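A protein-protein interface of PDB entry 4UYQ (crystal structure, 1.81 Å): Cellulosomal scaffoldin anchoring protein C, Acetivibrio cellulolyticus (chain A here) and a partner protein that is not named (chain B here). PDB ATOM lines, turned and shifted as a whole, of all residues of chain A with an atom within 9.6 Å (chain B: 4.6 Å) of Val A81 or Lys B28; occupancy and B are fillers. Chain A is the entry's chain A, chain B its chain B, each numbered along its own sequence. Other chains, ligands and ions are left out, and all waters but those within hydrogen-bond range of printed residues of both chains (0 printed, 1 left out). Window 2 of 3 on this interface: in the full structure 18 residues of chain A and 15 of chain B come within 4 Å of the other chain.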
ATOM      1  N   TYR A  32      22.069  14.445   0.168  1.00  0.00           N
ATOM      2  CA  TYR A  32      21.907  15.836   0.525  1.00  0.00           C
ATOM      3  C   TYR A  32      22.538  16.728  -0.547  1.00  0.00           C
ATOM      4  O   TYR A  32      22.041  17.813  -0.837  1.00  0.00           O
ATOM      5  CB  TYR A  32      22.553  16.026   1.888  1.00  0.00           C
ATOM      6  CG  TYR A  32      22.517  17.408   2.441  1.00  0.00           C
ATOM      7  CD1 TYR A  32      21.309  17.969   2.846  1.00  0.00           C
ATOM      8  CD2 TYR A  32      23.677  18.108   2.683  1.00  0.00           C
ATOM      9  CE1 TYR A  32      21.234  19.227   3.486  1.00  0.00           C
ATOM     10  CE2 TYR A  32      23.604  19.358   3.344  1.00  0.00           C
ATOM     11  CZ  TYR A  32      22.378  19.903   3.723  1.00  0.00           C
ATOM     12  OH  TYR A  32      22.235  21.156   4.324  1.00  0.00           O
ATOM     13  N   SER A  60      15.287  25.008  -8.300  1.00  0.00           N
ATOM     14  CA  SER A  60      16.262  25.791  -7.542  1.00  0.00           C
ATOM     15  C   SER A  60      17.353  24.945  -6.867  1.00  0.00           C
ATOM     16  O   SER A  60      18.421  25.436  -6.570  1.00  0.00           O
ATOM     17  CB  SER A  60      15.582  26.767  -6.567  1.00  0.00           C
ATOM     18  OG  SER A  60      15.242  26.138  -5.359  1.00  0.00           O
ATOM     19  N   ASP A  61      17.112  23.648  -6.711  1.00  0.00           N
ATOM     20  CA  ASP A  61      18.084  22.750  -6.097  1.00  0.00           C
ATOM     21  C   ASP A  61      19.159  22.242  -7.088  1.00  0.00           C
ATOM     22  O   ASP A  61      20.177  21.677  -6.631  1.00  0.00           O
ATOM     23  CB  ASP A  61      17.343  21.531  -5.491  1.00  0.00           C
ATOM     24  CG  ASP A  61      16.331  21.894  -4.377  1.00  0.00           C
ATOM     25  OD1 ASP A  61      16.474  22.978  -3.747  1.00  0.00           O
ATOM     26  OD2 ASP A  61      15.437  21.054  -4.097  1.00  0.00           O
ATOM     27  N   PHE A  77      23.300  18.999  -7.462  1.00  0.00           N
ATOM     28  CA  PHE A  77      22.124  19.046  -6.602  1.00  0.00           C
ATOM     29  C   PHE A  77      22.510  19.413  -5.206  1.00  0.00           C
ATOM     30  O   PHE A  77      23.467  18.820  -4.610  1.00  0.00           O
ATOM     31  CB  PHE A  77      21.386  17.691  -6.591  1.00  0.00           C
ATOM     32  CG  PHE A  77      20.285  17.597  -5.606  1.00  0.00           C
ATOM     33  CD1 PHE A  77      19.064  18.160  -5.890  1.00  0.00           C
ATOM     34  CD2 PHE A  77      20.437  16.871  -4.457  1.00  0.00           C
ATOM     35  CE1 PHE A  77      18.023  18.072  -4.986  1.00  0.00           C
ATOM     36  CE2 PHE A  77      19.406  16.774  -3.525  1.00  0.00           C
ATOM     37  CZ  PHE A  77      18.207  17.379  -3.803  1.00  0.00           C
ATOM     38  N   GLU A  78      21.763  20.342  -4.615  1.00  0.00           N
ATOM     39  CA  GLU A  78      21.963  20.750  -3.240  1.00  0.00           C
ATOM     40  C   GLU A  78      20.573  20.776  -2.562  1.00  0.00           C
ATOM     41  O   GLU A  78      19.707  21.593  -2.915  1.00  0.00           O
ATOM     42  CB  GLU A  78      22.575  22.154  -3.184  1.00  0.00           C
ATOM     43  CG  GLU A  78      23.857  22.362  -4.040  1.00  0.00           C
ATOM     44  CD  GLU A  78      24.086  23.803  -4.430  1.00  0.00           C
ATOM     45  OE1 GLU A  78      23.256  24.386  -5.232  1.00  0.00           O
ATOM     46  OE2 GLU A  78      25.136  24.348  -3.936  1.00  0.00           O
ATOM     47  N   ALA A  79      20.346  19.894  -1.620  1.00  0.00           N
ATOM     48  CA  ALA A  79      19.037  19.898  -0.907  1.00  0.00           C
ATOM     49  C   ALA A  79      18.944  21.157  -0.074  1.00  0.00           C
ATOM     50  O   ALA A  79      19.968  21.729   0.338  1.00  0.00           O
ATOM     51  CB  ALA A  79      18.917  18.742   0.067  1.00  0.00           C
ATOM     52  N   PRO A  80      17.727  21.596   0.191  1.00  0.00           N
ATOM     53  CA  PRO A  80      17.548  22.704   1.125  1.00  0.00           C
ATOM     54  C   PRO A  80      18.050  22.391   2.507  1.00  0.00           C
ATOM     55  O   PRO A  80      18.043  21.259   2.936  1.00  0.00           O
ATOM     56  CB  PRO A  80      16.036  22.902   1.126  1.00  0.00           C
ATOM     57  CG  PRO A  80      15.443  21.587   0.699  1.00  0.00           C
ATOM     58  CD  PRO A  80      16.424  21.121  -0.346  1.00  0.00           C
ATOM     59  N   VAL A  81      18.438  23.429   3.247  1.00  0.00           N
ATOM     60  CA  VAL A  81      19.086  23.212   4.542  1.00  0.00           C
ATOM     61  C   VAL A  81      18.080  22.532   5.520  1.00  0.00           C
ATOM     62  O   VAL A  81      18.482  21.731   6.335  1.00  0.00           O
ATOM     63  CB  VAL A  81      19.685  24.500   5.126  1.00  0.00           C
ATOM     64  CG1 VAL A  81      18.604  25.439   5.583  1.00  0.00           C
ATOM     65  CG2 VAL A  81      20.641  24.195   6.298  1.00  0.00           C
ATOM     66  N   ASP A  82      16.783  22.759   5.361  1.00  0.00           N
ATOM     67  CA  ASP A  82      15.805  22.074   6.266  1.00  0.00           C
ATOM     68  C   ASP A  82      15.478  20.594   5.826  1.00  0.00           C
ATOM     69  O   ASP A  82      14.626  19.893   6.397  1.00  0.00           O
ATOM     70  CB  ASP A  82      14.537  22.944   6.408  1.00  0.00           C
ATOM     71  CG  ASP A  82      13.699  23.034   5.107  1.00  0.00           C
ATOM     72  OD1 ASP A  82      14.029  22.412   4.083  1.00  0.00           O
ATOM     73  OD2 ASP A  82      12.695  23.769   5.097  1.00  0.00           O
ATOM     74  N   ARG A  83      16.184  20.109   4.791  1.00  0.00           N
ATOM     75  CA  ARG A  83      16.005  18.753   4.265  1.00  0.00           C
ATOM     76  C   ARG A  83      14.523  18.509   3.868  1.00  0.00           C
ATOM     77  O   ARG A  83      14.075  17.399   3.892  1.00  0.00           O
ATOM     78  CB  ARG A  83      16.652  17.663   5.198  1.00  0.00           C
ATOM     79  CG  ARG A  83      18.134  17.977   5.415  1.00  0.00           C
ATOM     80  CD  ARG A  83      19.020  17.204   6.416  1.00  0.00           C
ATOM     81  NE  ARG A  83      19.053  15.853   5.979  1.00  0.00           N
ATOM     82  CZ  ARG A  83      20.076  15.158   5.550  1.00  0.00           C
ATOM     83  NH1 ARG A  83      21.386  15.589   5.605  1.00  0.00           N
ATOM     84  NH2 ARG A  83      19.777  13.960   5.168  1.00  0.00           N
ATOM     85  N   ALA A  84      13.791  19.525   3.442  1.00  0.00           N
ATOM     86  CA  ALA A  84      12.415  19.306   2.921  1.00  0.00           C
ATOM     87  C   ALA A  84      12.329  18.482   1.606  1.00  0.00           C
ATOM     88  O   ALA A  84      11.275  17.917   1.285  1.00  0.00           O
ATOM     89  CB  ALA A  84      11.709  20.639   2.695  1.00  0.00           C
ATOM     90  N   ARG A  85      13.419  18.427   0.849  1.00  0.00           N
ATOM     91  CA  ARG A  85      13.460  17.773  -0.439  1.00  0.00           C
ATOM     92  C   ARG A  85      14.799  17.126  -0.310  1.00  0.00           C
ATOM     93  O   ARG A  85      15.709  17.750   0.193  1.00  0.00           O
ATOM     94  CB  ARG A  85      13.460  18.783  -1.561  1.00  0.00           C
ATOM     95  CG  ARG A  85      12.137  19.594  -1.591  1.00  0.00           C
ATOM     96  CD  ARG A  85      12.168  20.574  -2.728  1.00  0.00           C
ATOM     97  NE  ARG A  85      13.229  21.561  -2.624  1.00  0.00           N
ATOM     98  CZ  ARG A  85      13.152  22.718  -1.983  1.00  0.00           C
ATOM     99  NH1 ARG A  85      12.063  23.027  -1.321  1.00  0.00           N
ATOM    100  NH2 ARG A  85      14.144  23.597  -2.055  1.00  0.00           N
ATOM    101  N   ILE A  86      14.902  15.874  -0.655  1.00  0.00           N
ATOM    102  CA  ILE A  86      16.186  15.146  -0.581  1.00  0.00           C
ATOM    103  C   ILE A  86      15.985  14.016  -1.601  1.00  0.00           C
ATOM    104  O   ILE A  86      14.866  13.610  -1.794  1.00  0.00           O
ATOM    105  CB  ILE A  86      16.491  14.673   0.817  1.00  0.00           C
ATOM    106  CG1 ILE A  86      17.867  14.058   0.863  1.00  0.00           C
ATOM    107  CG2 ILE A  86      15.540  13.653   1.342  1.00  0.00           C
ATOM    108  CD1 ILE A  86      18.589  14.480   2.115  1.00  0.00           C
ATOM    109  N   SER A 124      25.368  14.233   3.813  1.00  0.00           N
ATOM    110  CA  SER A 124      25.304  15.429   4.678  1.00  0.00           C
ATOM    111  C   SER A 124      26.452  16.327   4.283  1.00  0.00           C
ATOM    112  O   SER A 124      27.260  15.946   3.416  1.00  0.00           O
ATOM    113  CB  SER A 124      25.433  15.085   6.166  1.00  0.00           C
ATOM    114  OG  SER A 124      26.717  14.638   6.467  1.00  0.00           O
ATOM    115  N   GLY A 125      26.586  17.466   4.939  1.00  0.00           N
ATOM    116  CA  GLY A 125      27.691  18.374   4.616  1.00  0.00           C
ATOM    117  C   GLY A 125      29.076  17.798   4.823  1.00  0.00           C
ATOM    118  O   GLY A 125      29.999  18.175   4.132  1.00  0.00           O
ATOM    119  N   ARG B  22      27.271  27.394   2.567  1.00  0.00           N
ATOM    120  CA  ARG B  22      25.893  27.831   2.578  1.00  0.00           C
ATOM    121  C   ARG B  22      25.282  27.608   3.984  1.00  0.00           C
ATOM    122  O   ARG B  22      24.606  28.526   4.537  1.00  0.00           O
ATOM    123  CB  ARG B  22      25.112  27.075   1.535  1.00  0.00           C
ATOM    124  CG  ARG B  22      23.650  27.474   1.576  1.00  0.00           C
ATOM    125  CD  ARG B  22      22.721  26.416   0.976  1.00  0.00           C
ATOM    126  NE  ARG B  22      22.661  25.149   1.705  1.00  0.00           N
ATOM    127  CZ  ARG B  22      21.873  24.155   1.333  1.00  0.00           C
ATOM    128  NH1 ARG B  22      21.223  24.272   0.185  1.00  0.00           N
ATOM    129  NH2 ARG B  22      21.830  23.002   2.017  1.00  0.00           N
ATOM    130  N   ASP B  23      25.526  26.435   4.572  1.00  0.00           N
ATOM    131  CA  ASP B  23      24.958  26.069   5.863  1.00  0.00           C
ATOM    132  C   ASP B  23      25.569  26.931   7.008  1.00  0.00           C
ATOM    133  O   ASP B  23      24.902  27.291   8.025  1.00  0.00           O
ATOM    134  CB  ASP B  23      25.119  24.552   6.136  1.00  0.00           C
ATOM    135  CG  ASP B  23      24.234  23.648   5.187  1.00  0.00           C
ATOM    136  OD1 ASP B  23      23.456  24.146   4.300  1.00  0.00           O
ATOM    137  OD2 ASP B  23      24.383  22.415   5.306  1.00  0.00           O
ATOM    138  N   LEU B  26      23.823  30.385   6.692  1.00  0.00           N
ATOM    139  CA  LEU B  26      22.455  30.287   7.168  1.00  0.00           C
ATOM    140  C   LEU B  26      22.339  30.037   8.661  1.00  0.00           C
ATOM    141  O   LEU B  26      21.252  29.978   9.168  1.00  0.00           O
ATOM    142  CB  LEU B  26      21.670  29.232   6.406  1.00  0.00           C
ATOM    143  CG  LEU B  26      21.440  29.536   4.924  1.00  0.00           C
ATOM    144  CD1 LEU B  26      20.886  28.307   4.230  1.00  0.00           C
ATOM    145  CD2 LEU B  26      20.524  30.720   4.645  1.00  0.00           C
ATOM    146  N   GLY B  27      23.449  29.879   9.353  1.00  0.00           N
ATOM    147  CA  GLY B  27      23.448  29.627  10.759  1.00  0.00           C
ATOM    148  C   GLY B  27      23.132  28.214  11.166  1.00  0.00           C
ATOM    149  O   GLY B  27      22.815  27.984  12.323  1.00  0.00           O
ATOM    150  N   LYS B  28      23.287  27.239  10.257  1.00  0.00           N
ATOM    151  CA  LYS B  28      22.970  25.848  10.583  1.00  0.00           C
ATOM    152  C   LYS B  28      24.149  25.238  11.297  1.00  0.00           C
ATOM    153  O   LYS B  28      23.999  24.419  12.183  1.00  0.00           O
ATOM    154  CB  LYS B  28      22.552  25.081   9.323  1.00  0.00           C
ATOM    155  CG  LYS B  28      22.430  23.546   9.396  1.00  0.00           C
ATOM    156  CD  LYS B  28      21.444  23.093  10.471  1.00  0.00           C
ATOM    157  CE  LYS B  28      20.758  21.755  10.161  1.00  0.00           C
ATOM    158  NZ  LYS B  28      19.320  21.925   9.751  1.00  0.00           N
ATOM    159  N   ILE B  29      25.340  25.695  10.946  1.00  0.00           N
ATOM    160  CA  ILE B  29      26.568  25.284  11.596  1.00  0.00           C
ATOM    161  C   ILE B  29      27.278  26.572  11.933  1.00  0.00           C
ATOM    162  O   ILE B  29      27.041  27.615  11.316  1.00  0.00           O
ATOM    163  CB  ILE B  29      27.460  24.376  10.675  1.00  0.00           C
ATOM    164  CG1 ILE B  29      27.994  25.159   9.482  1.00  0.00           C
ATOM    165  CG2 ILE B  29      26.650  23.190  10.146  1.00  0.00           C
ATOM    166  CD1 ILE B  29      28.915  24.332   8.586  1.00  0.00           C
ATOM    167  N   ASN B  30      28.164  26.481  12.891  1.00  0.00           N
ATOM    168  CA  ASN B  30      28.870  27.640  13.469  1.00  0.00           C
ATOM    169  C   ASN B  30      30.371  27.687  13.244  1.00  0.00           C
ATOM    170  O   ASN B  30      31.005  28.671  13.573  1.00  0.00           O
ATOM    171  CB  ASN B  30      28.614  27.657  14.965  1.00  0.00           C
ATOM    172  CG  ASN B  30      27.171  27.934  15.252  1.00  0.00           C
ATOM    173  OD1 ASN B  30      26.624  28.928  14.751  1.00  0.00           O
ATOM    174  ND2 ASN B  30      26.516  27.033  15.971  1.00  0.00           N
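The backbone carbonyl oxygen (O) of Asp B23 lies within hydrogen-bond range of the backbone NH (N) of Ile B29, at 3.4 Å. O of Asp B23 sits at hydrogen-bond distance from N of Lys B28 (2.8 Å). The backbone carbonyl oxygen (O) of Tyr A32 sits at hydrogen-bond distance from the backbone NH (N) of Ala A79, at 2.8 Å. NE of Arg B22 lies within salt-bridge range of OD1 of Asp B23 (2.9 Å).
Among the printed residues, pairs that only touch across the chains: Pro A80 with Arg B22 (3.9 Å), Val A81 with Arg B22 (3.6 Å), Val A81 with Asp B23 (3.5 Å), Val A81 with Leu B26 (3.9 Å) and Val A81 with Lys B28 (3.5 Å).
Val A81 touches just these residues of chain B: Arg B22 (3.6 Å), Asp B23 (3.5 Å), Leu B26 (3.9 Å) and Lys B28 (3.5 Å). Of chain A, only Val A81 (3.5 Å) comes within 4 Å of Lys B28. No residue of chain A comes within 4 Å of Gly B27. Of the printed residues of chain A, Asp B23 touches Tyr A32 (2.7 Å) and Val A81 (3.5 Å). Of the printed residues of chain B, Tyr A32 touches Arg B22 and Asp B23. Ile A86 touches none of the printed residues of chain B. The nearest printed residue of chain B that does not touch Val A81 is Ile B29 (6.8 Å). The nearest printed residue of chain A that does not touch Arg B22 is Glu A78 (4.2 Å).
Printed residues of chain B that touch a printed residue of chain A: Arg B22, Asp B23, Leu B26 and Lys B28. Among the printed residues, 8 pairs touch across the chains.
The side-chain hydroxyl of Tyr A32 is in hydrogen-bond range of the guanidinium group of Arg B22 (3.0 Å). OH of Tyr A32 lies within hydrogen-bond range of OD2 of Asp B23. The backbone carbonyl oxygen (O) of Ala A79 sits at hydrogen-bond distance from the guanidinium group (NH2) of Arg B22 (2.8 Å).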
